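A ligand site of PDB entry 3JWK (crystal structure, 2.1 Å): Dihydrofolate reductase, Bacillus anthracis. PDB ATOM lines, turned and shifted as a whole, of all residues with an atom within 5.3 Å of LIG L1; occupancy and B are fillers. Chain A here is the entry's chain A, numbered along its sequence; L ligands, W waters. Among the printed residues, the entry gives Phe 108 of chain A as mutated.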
ATOM      1  N   MET A  12      10.352  15.465  -7.607  1.00  0.00           N
ATOM      2  CA  MET A  12      10.652  16.363  -6.509  1.00  0.00           C
ATOM      3  C   MET A  12      10.834  15.538  -5.240  1.00  0.00           C
ATOM      4  O   MET A  12       9.903  14.890  -4.788  1.00  0.00           O
ATOM      5  CB  MET A  12       9.544  17.410  -6.365  1.00  0.00           C
ATOM      6  CG  MET A  12       9.614  18.260  -5.086  1.00  0.00           C
ATOM      7  SD  MET A  12      10.986  19.416  -4.988  1.00  0.00           S
ATOM      8  CE  MET A  12      10.537  20.571  -6.297  1.00  0.00           C
ATOM      9  N   VAL A  13      12.046  15.546  -4.677  1.00  0.00           N
ATOM     10  CA  VAL A  13      12.403  14.687  -3.539  1.00  0.00           C
ATOM     11  C   VAL A  13      13.443  15.333  -2.622  1.00  0.00           C
ATOM     12  O   VAL A  13      14.303  16.067  -3.068  1.00  0.00           O
ATOM     13  CB  VAL A  13      12.870  13.263  -4.015  1.00  0.00           C
ATOM     14  CG1 VAL A  13      14.134  13.319  -4.857  1.00  0.00           C
ATOM     15  CG2 VAL A  13      13.059  12.301  -2.837  1.00  0.00           C
ATOM     16  N   ALA A  14      13.335  15.066  -1.323  1.00  0.00           N
ATOM     17  CA  ALA A  14      14.395  15.393  -0.377  1.00  0.00           C
ATOM     18  C   ALA A  14      14.901  14.081   0.231  1.00  0.00           C
ATOM     19  O   ALA A  14      14.108  13.279   0.731  1.00  0.00           O
ATOM     20  CB  ALA A  14      13.873  16.332   0.726  1.00  0.00           C
ATOM     21  N   ASN A  26       6.377   8.981   7.913  1.00  0.00           N
ATOM     22  CA  ASN A  26       6.541  10.418   8.086  1.00  0.00           C
ATOM     23  C   ASN A  26       7.909  10.858   7.570  1.00  0.00           C
ATOM     24  O   ASN A  26       8.762  10.004   7.273  1.00  0.00           O
ATOM     25  CB  ASN A  26       6.393  10.791   9.571  1.00  0.00           C
ATOM     26  CG  ASN A  26       4.944  10.792  10.046  1.00  0.00           C
ATOM     27  OD1 ASN A  26       4.082  11.467   9.477  1.00  0.00           O
ATOM     28  ND2 ASN A  26       4.675  10.026  11.106  1.00  0.00           N
ATOM     29  N   LEU A  27       8.117  12.158   7.486  1.00  0.00           N
ATOM     30  CA  LEU A  27       9.394  12.762   7.138  1.00  0.00           C
ATOM     31  C   LEU A  27      10.308  12.714   8.362  1.00  0.00           C
ATOM     32  O   LEU A  27       9.869  13.084   9.454  1.00  0.00           O
ATOM     33  CB  LEU A  27       9.122  14.210   6.727  1.00  0.00           C
ATOM     34  CG  LEU A  27       9.857  14.968   5.630  1.00  0.00           C
ATOM     35  CD1 LEU A  27      10.201  14.106   4.427  1.00  0.00           C
ATOM     36  CD2 LEU A  27       8.974  16.162   5.237  1.00  0.00           C
ATOM     37  N   GLU A  34      13.131  24.337   3.318  1.00  0.00           N
ATOM     38  CA  GLU A  34      13.086  23.362   2.241  1.00  0.00           C
ATOM     39  C   GLU A  34      11.662  23.256   1.672  1.00  0.00           C
ATOM     40  O   GLU A  34      11.471  23.191   0.457  1.00  0.00           O
ATOM     41  CB  GLU A  34      13.600  22.011   2.724  1.00  0.00           C
ATOM     42  CG  GLU A  34      14.242  21.134   1.646  1.00  0.00           C
ATOM     43  CD  GLU A  34      13.234  20.360   0.799  1.00  0.00           C
ATOM     44  OE1 GLU A  34      12.212  19.867   1.345  1.00  0.00           O
ATOM     45  OE2 GLU A  34      13.464  20.217  -0.420  1.00  0.00           O
ATOM     46  N   LEU A  35      10.670  23.250   2.553  1.00  0.00           N
ATOM     47  CA  LEU A  35       9.261  23.282   2.129  1.00  0.00           C
ATOM     48  C   LEU A  35       8.901  24.519   1.321  1.00  0.00           C
ATOM     49  O   LEU A  35       8.082  24.424   0.407  1.00  0.00           O
ATOM     50  CB  LEU A  35       8.329  23.148   3.356  1.00  0.00           C
ATOM     51  CG  LEU A  35       7.868  21.739   3.782  1.00  0.00           C
ATOM     52  CD1 LEU A  35       9.018  20.770   3.933  1.00  0.00           C
ATOM     53  CD2 LEU A  35       7.053  21.796   5.084  1.00  0.00           C
ATOM     54  N   VAL A  38      10.085  23.917  -2.116  1.00  0.00           N
ATOM     55  CA  VAL A  38       9.140  22.972  -2.729  1.00  0.00           C
ATOM     56  C   VAL A  38       7.877  23.683  -3.276  1.00  0.00           C
ATOM     57  O   VAL A  38       7.483  23.460  -4.424  1.00  0.00           O
ATOM     58  CB  VAL A  38       8.717  21.858  -1.746  1.00  0.00           C
ATOM     59  CG1 VAL A  38       7.580  20.999  -2.330  1.00  0.00           C
ATOM     60  CG2 VAL A  38       9.919  20.971  -1.381  1.00  0.00           C
ATOM     61  N   ASN A  53       1.660   8.749   0.859  1.00  0.00           N
ATOM     62  CA  ASN A  53       2.140  10.132   0.886  1.00  0.00           C
ATOM     63  C   ASN A  53       0.964  11.109   1.064  1.00  0.00           C
ATOM     64  O   ASN A  53       0.993  11.939   1.978  1.00  0.00           O
ATOM     65  CB  ASN A  53       2.919  10.449  -0.403  1.00  0.00           C
ATOM     66  CG  ASN A  53       3.401  11.920  -0.483  1.00  0.00           C
ATOM     67  OD1 ASN A  53       3.523  12.595   0.524  1.00  0.00           O
ATOM     68  ND2 ASN A  53       3.689  12.371  -1.694  1.00  0.00           N
ATOM     69  N   ALA A  56      -0.940  11.091   4.650  1.00  0.00           N
ATOM     70  CA  ALA A  56      -0.180  11.732   5.718  1.00  0.00           C
ATOM     71  C   ALA A  56      -0.303  13.264   5.652  1.00  0.00           C
ATOM     72  O   ALA A  56      -0.213  13.933   6.684  1.00  0.00           O
ATOM     73  CB  ALA A  56       1.274  11.317   5.669  1.00  0.00           C
ATOM     74  N   ILE A  57      -0.467  13.799   4.442  1.00  0.00           N
ATOM     75  CA  ILE A  57      -0.743  15.231   4.259  1.00  0.00           C
ATOM     76  C   ILE A  57      -2.186  15.522   4.676  1.00  0.00           C
ATOM     77  O   ILE A  57      -2.436  16.455   5.434  1.00  0.00           O
ATOM     78  CB  ILE A  57      -0.472  15.707   2.782  1.00  0.00           C
ATOM     79  CG1 ILE A  57       0.989  15.481   2.390  1.00  0.00           C
ATOM     80  CG2 ILE A  57      -0.853  17.187   2.612  1.00  0.00           C
ATOM     81  CD1 ILE A  57       1.320  15.699   0.912  1.00  0.00           C
ATOM     82  N   LEU A  61      -2.905  20.255  -1.461  1.00  0.00           N
ATOM     83  CA  LEU A  61      -1.970  21.373  -1.459  1.00  0.00           C
ATOM     84  C   LEU A  61      -2.495  22.437  -2.448  1.00  0.00           C
ATOM     85  O   LEU A  61      -2.837  22.101  -3.578  1.00  0.00           O
ATOM     86  CB  LEU A  61      -0.563  20.909  -1.860  1.00  0.00           C
ATOM     87  CG  LEU A  61       0.190  19.983  -0.895  1.00  0.00           C
ATOM     88  CD1 LEU A  61       1.578  19.705  -1.439  1.00  0.00           C
ATOM     89  CD2 LEU A  61       0.301  20.555   0.525  1.00  0.00           C
ATOM     90  N   PHE A 102       5.862  13.370  -6.695  1.00  0.00           N
ATOM     91  CA  PHE A 102       6.044  13.989  -5.376  1.00  0.00           C
ATOM     92  C   PHE A 102       6.281  12.924  -4.293  1.00  0.00           C
ATOM     93  O   PHE A 102       6.488  13.265  -3.120  1.00  0.00           O
ATOM     94  CB  PHE A 102       4.781  14.815  -5.070  1.00  0.00           C
ATOM     95  CG  PHE A 102       4.986  15.974  -4.115  1.00  0.00           C
ATOM     96  CD1 PHE A 102       5.951  16.939  -4.341  1.00  0.00           C
ATOM     97  CD2 PHE A 102       4.139  16.119  -3.021  1.00  0.00           C
ATOM     98  CE1 PHE A 102       6.108  18.014  -3.467  1.00  0.00           C
ATOM     99  CE2 PHE A 102       4.277  17.187  -2.132  1.00  0.00           C
ATOM    100  CZ  PHE A 102       5.264  18.146  -2.367  1.00  0.00           C
ATOM    101  N   GLY A 103       6.277  11.648  -4.688  1.00  0.00           N
ATOM    102  CA  GLY A 103       6.522  10.535  -3.749  1.00  0.00           C
ATOM    103  C   GLY A 103       5.265   9.851  -3.220  1.00  0.00           C
ATOM    104  O   GLY A 103       4.145  10.238  -3.583  1.00  0.00           O
ATOM    105  N   PHE A 108       7.754   6.929  -6.659  1.00  0.00           N
ATOM    106  CA  PHE A 108       9.022   7.233  -7.353  1.00  0.00           C
ATOM    107  C   PHE A 108       9.507   6.030  -8.199  1.00  0.00           C
ATOM    108  O   PHE A 108       9.945   6.224  -9.346  1.00  0.00           O
ATOM    109  CB  PHE A 108      10.118   7.644  -6.370  1.00  0.00           C
ATOM    110  CG  PHE A 108       9.951   9.020  -5.754  1.00  0.00           C
ATOM    111  CD1 PHE A 108      10.137   9.186  -4.387  1.00  0.00           C
ATOM    112  CD2 PHE A 108       9.659  10.139  -6.530  1.00  0.00           C
ATOM    113  CE1 PHE A 108      10.016  10.448  -3.785  1.00  0.00           C
ATOM    114  CE2 PHE A 108       9.539  11.397  -5.937  1.00  0.00           C
ATOM    115  CZ  PHE A 108       9.720  11.551  -4.575  1.00  0.00           C
ATOM    116  N   TYR A 119      14.565  17.246  -9.329  1.00  0.00           N
ATOM    117  CA  TYR A 119      14.789  18.270  -8.311  1.00  0.00           C
ATOM    118  C   TYR A 119      14.998  17.543  -6.989  1.00  0.00           C
ATOM    119  O   TYR A 119      14.024  17.122  -6.334  1.00  0.00           O
ATOM    120  CB  TYR A 119      13.603  19.231  -8.180  1.00  0.00           C
ATOM    121  CG  TYR A 119      13.198  19.993  -9.427  1.00  0.00           C
ATOM    122  CD1 TYR A 119      12.514  19.360 -10.456  1.00  0.00           C
ATOM    123  CD2 TYR A 119      13.456  21.366  -9.557  1.00  0.00           C
ATOM    124  CE1 TYR A 119      12.130  20.056 -11.595  1.00  0.00           C
ATOM    125  CE2 TYR A 119      13.065  22.087 -10.707  1.00  0.00           C
ATOM    126  CZ  TYR A 119      12.396  21.409 -11.704  1.00  0.00           C
ATOM    127  OH  TYR A 119      11.992  22.062 -12.855  1.00  0.00           O
ATOM    128  N   THR A 121      16.777  17.501  -3.162  1.00  0.00           N
ATOM    129  CA  THR A 121      17.442  18.136  -2.046  1.00  0.00           C
ATOM    130  C   THR A 121      18.257  17.062  -1.333  1.00  0.00           C
ATOM    131  O   THR A 121      17.737  16.003  -1.004  1.00  0.00           O
ATOM    132  CB  THR A 121      16.432  18.760  -1.052  1.00  0.00           C
ATOM    133  OG1 THR A 121      15.629  19.735  -1.741  1.00  0.00           O
ATOM    134  CG2 THR A 121      17.170  19.425   0.115  1.00  0.00           C
HETATM  135  N1  LIG L   1      10.749  18.013  -0.092  1.00  0.00           N
HETATM  136  C1  LIG L   1      11.097  17.743  -1.363  1.00  0.00           C
HETATM  137  N2  LIG L   1      10.335  16.964  -2.134  1.00  0.00           N
HETATM  138  C2  LIG L   1       9.185  16.420  -1.651  1.00  0.00           C
HETATM  139  C3  LIG L   1       8.813  16.688  -0.334  1.00  0.00           C
HETATM  140  C4  LIG L   1       9.632  17.509   0.439  1.00  0.00           C
HETATM  141  C5  LIG L   1       4.420  20.250   1.078  1.00  0.00           C
HETATM  142  C6  LIG L   1       3.645  14.993   5.948  1.00  0.00           C
HETATM  143  C7  LIG L   1       2.060  19.752   4.499  1.00  0.00           C
HETATM  144  C8  LIG L   1       6.690  13.921   3.022  1.00  0.00           C
HETATM  145  C9  LIG L   1       9.258  17.833   1.895  1.00  0.00           C
HETATM  146  N3  LIG L   1      12.220  18.281  -1.844  1.00  0.00           N
HETATM  147  N4  LIG L   1       8.426  15.629  -2.416  1.00  0.00           N
HETATM  148  C10 LIG L   1       7.605  16.149   0.215  1.00  0.00           C
HETATM  149  C11 LIG L   1       6.610  15.707   0.715  1.00  0.00           C
HETATM  150  C12 LIG L   1       4.643  17.609   1.874  1.00  0.00           C
HETATM  151  C13 LIG L   1       4.505  15.940   3.600  1.00  0.00           C
HETATM  152  O1  LIG L   1       3.957  19.881   2.386  1.00  0.00           O
HETATM  153  O2  LIG L   1       3.689  16.443   5.774  1.00  0.00           O
HETATM  154  O3  LIG L   1       3.317  19.137   4.945  1.00  0.00           O
HETATM  155  O4  LIG L   1       5.551  13.952   2.131  1.00  0.00           O
HETATM  156  C14 LIG L   1       4.842  16.292   2.302  1.00  0.00           C
HETATM  157  C15 LIG L   1       4.148  18.572   2.766  1.00  0.00           C
HETATM  158  C16 LIG L   1       3.998  16.863   4.500  1.00  0.00           C
HETATM  159  C17 LIG L   1       3.818  18.195   4.076  1.00  0.00           C
HETATM  160  C18 LIG L   1       5.379  15.195   1.372  1.00  0.00           C
HETATM  161  P1  LG2 L   2       3.665   5.918  -1.434  1.00  0.00           P
HETATM  162  O1  LG2 L   2       4.556   5.598  -2.569  1.00  0.00           O
HETATM  163  O2  LG2 L   2       3.505   7.357  -1.157  1.00  0.00           O
HETATM  164  O3  LG2 L   2       2.230   5.256  -1.631  1.00  0.00           O
HETATM  165  C1  LG2 L   2       2.084   3.862  -1.636  1.00  0.00           C
HETATM  166  C2  LG2 L   2       0.733   3.603  -2.267  1.00  0.00           C
HETATM  167  O4  LG2 L   2       0.738   4.027  -3.615  1.00  0.00           O
HETATM  168  C3  LG2 L   2       0.368   2.127  -2.308  1.00  0.00           C
HETATM  169  O5  LG2 L   2      -0.089   1.708  -1.043  1.00  0.00           O
HETATM  170  C4  LG2 L   2      -0.693   2.158  -3.388  1.00  0.00           C
HETATM  171  O6  LG2 L   2      -1.920   2.642  -2.867  1.00  0.00           O
HETATM  172  C5  LG2 L   2      -0.126   3.198  -4.361  1.00  0.00           C
HETATM  173  N1  LG2 L   2       0.596   2.464  -5.409  1.00  0.00           N
HETATM  174  C6  LG2 L   2       1.861   1.915  -5.348  1.00  0.00           C
HETATM  175  N2  LG2 L   2       2.130   1.296  -6.520  1.00  0.00           N
HETATM  176  C7  LG2 L   2       1.055   1.439  -7.332  1.00  0.00           C
HETATM  177  C8  LG2 L   2       0.777   1.022  -8.624  1.00  0.00           C
HETATM  178  N3  LG2 L   2       1.667   0.321  -9.325  1.00  0.00           N
HETATM  179  N4  LG2 L   2      -0.429   1.333  -9.182  1.00  0.00           N
HETATM  180  C9  LG2 L   2      -1.371   2.056  -8.502  1.00  0.00           C
HETATM  181  N5  LG2 L   2      -1.094   2.469  -7.219  1.00  0.00           N
HETATM  182  C10 LG2 L   2       0.091   2.168  -6.643  1.00  0.00           C
HETATM  183  O7  LG2 L   2       4.175   5.115  -0.136  1.00  0.00           O
HETATM  184  P2  LG2 L   2       5.614   4.803   0.463  1.00  0.00           P
HETATM  185  O8  LG2 L   2       5.382   4.097   1.749  1.00  0.00           O
HETATM  186  O9  LG2 L   2       6.494   4.236  -0.589  1.00  0.00           O
HETATM  187  O10 LG2 L   2       6.148   6.307   0.786  1.00  0.00           O
HETATM  188  C11 LG2 L   2       5.698   6.974   1.949  1.00  0.00           C
HETATM  189  C12 LG2 L   2       6.880   7.487   2.750  1.00  0.00           C
HETATM  190  O11 LG2 L   2       7.674   8.328   1.934  1.00  0.00           O
HETATM  191  C13 LG2 L   2       6.467   8.324   3.944  1.00  0.00           C
HETATM  192  O12 LG2 L   2       7.404   8.103   4.972  1.00  0.00           O
HETATM  193  C14 LG2 L   2       6.630   9.757   3.467  1.00  0.00           C
HETATM  194  O13 LG2 L   2       6.914  10.615   4.540  1.00  0.00           O
HETATM  195  C15 LG2 L   2       7.841   9.602   2.570  1.00  0.00           C
HETATM  196  N6  LG2 L   2       7.971  10.667   1.548  1.00  0.00           N
HETATM  197  C16 LG2 L   2       9.116  11.396   1.552  1.00  0.00           C
HETATM  198  C17 LG2 L   2       9.313  12.402   0.601  1.00  0.00           C
HETATM  199  C18 LG2 L   2      10.631  13.087   0.556  1.00  0.00           C
HETATM  200  O14 LG2 L   2      10.961  13.798  -0.590  1.00  0.00           O
HETATM  201  N7  LG2 L   2      11.471  13.032   1.586  1.00  0.00           N
HETATM  202  C19 LG2 L   2       8.332  12.650  -0.374  1.00  0.00           C
HETATM  203  C20 LG2 L   2       7.161  11.882  -0.359  1.00  0.00           C
HETATM  204  C21 LG2 L   2       6.983  10.896   0.605  1.00  0.00           C
HETATM  205  P3  LG2 L   2      -3.129   1.709  -2.365  1.00  0.00           P
HETATM  206  O15 LG2 L   2      -3.506   0.782  -3.493  1.00  0.00           O
HETATM  207  O16 LG2 L   2      -2.630   0.937  -1.148  1.00  0.00           O
HETATM  208  O17 LG2 L   2      -4.245   2.614  -1.966  1.00  0.00           O
HETATM  209  O   HOH W   1       3.509  12.597   3.176  1.00  0.00           O
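N of Asn 26 is in hydrogen-bond range of O12 of LG2 L2 (3.2 Å). The side-chain sulfur of Met 12 is in hydrogen-bond range of a nitrogen (N3) of LIG L1 (3.6 Å). O of Met 12 is in hydrogen-bond range of N4 of LIG L1. The side-chain carboxylate of Glu 34 lies within hydrogen-bond range of a nitrogen (N3) of LIG L1 (2.7 Å). The backbone carbonyl oxygen (O) of Phe 102 is in hydrogen-bond range of a nitrogen (N4) of LIG L1 (3.1 Å). OD1 of Asn 53 sits close to O4 of LIG L1. The backbone carbonyl oxygen of Asn 26 is in hydrogen-bond range of an oxygen (O12) of LG2 L2. The backbone NH (N) of Asn 53 lies within hydrogen-bond range of an oxygen (O2) of LG2 L2 (3.1 Å). An oxygen (O14) of LG2 L2 is in hydrogen-bond range of the backbone NH (N) of Ala 14 (2.8 Å). O of Val 13 lies within hydrogen-bond range of N3 of LIG L1 (3.3 Å). N2 of LIG L1 lies within hydrogen-bond range of N of Val 13 (3.4 Å). The backbone carbonyl oxygen (O) of Ala 14 sits at hydrogen-bond distance from a nitrogen (N7) of LG2 L2 (2.8 Å).
The side-chain hydroxyl (OG1) of Thr 121 is in hydrogen-bond range of the side-chain carboxylate (OE2) of Glu 34 (2.6 Å). The backbone carbonyl oxygen (O) of Val 13 sits at hydrogen-bond distance from the backbone NH (N) of Thr 121 (2.9 Å). The backbone carbonyl oxygen (O) of Tyr 119 is in hydrogen-bond range of the backbone NH (N) of Val 13, at 3.0 Å. The side-chain amide nitrogen (ND2) of Asn 53 is in hydrogen-bond range of the backbone carbonyl oxygen (O) of Gly 103 (2.9 Å). The side-chain amide nitrogen (ND2) of Asn 53 sits at hydrogen-bond distance from the backbone carbonyl oxygen (O) of Phe 102, at 3.3 Å.
The backbone NH of Ala 14 sits close to a nitrogen (N3) of LIG L1 (3.4 Å). Residues that only touch LIG L1: Leu 27 (3.7 Å), Leu 35 (3.6 Å), Val 38 (3.3 Å), Ile 57 (3.7 Å), Leu 61 (3.8 Å) and Thr 121 (3.7 Å). Hydrophobic or aromatic side chains that line LIG L1: Met 12, Ala 14, Leu 27, Leu 35, Val 38, Ile 57, Leu 61 and Phe 102. Of the 17 residues printed, 12 come within 4 Å of LIG L1. The nearest printed residue that does not touch LIG L1 is Ala 56 (4.1 Å).
Water W1 lies within hydrogen-bond range of the side-chain amide oxygen of Asn 53 (2.7 Å) and an oxygen (O4) of LIG L1 (2.7 Å).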
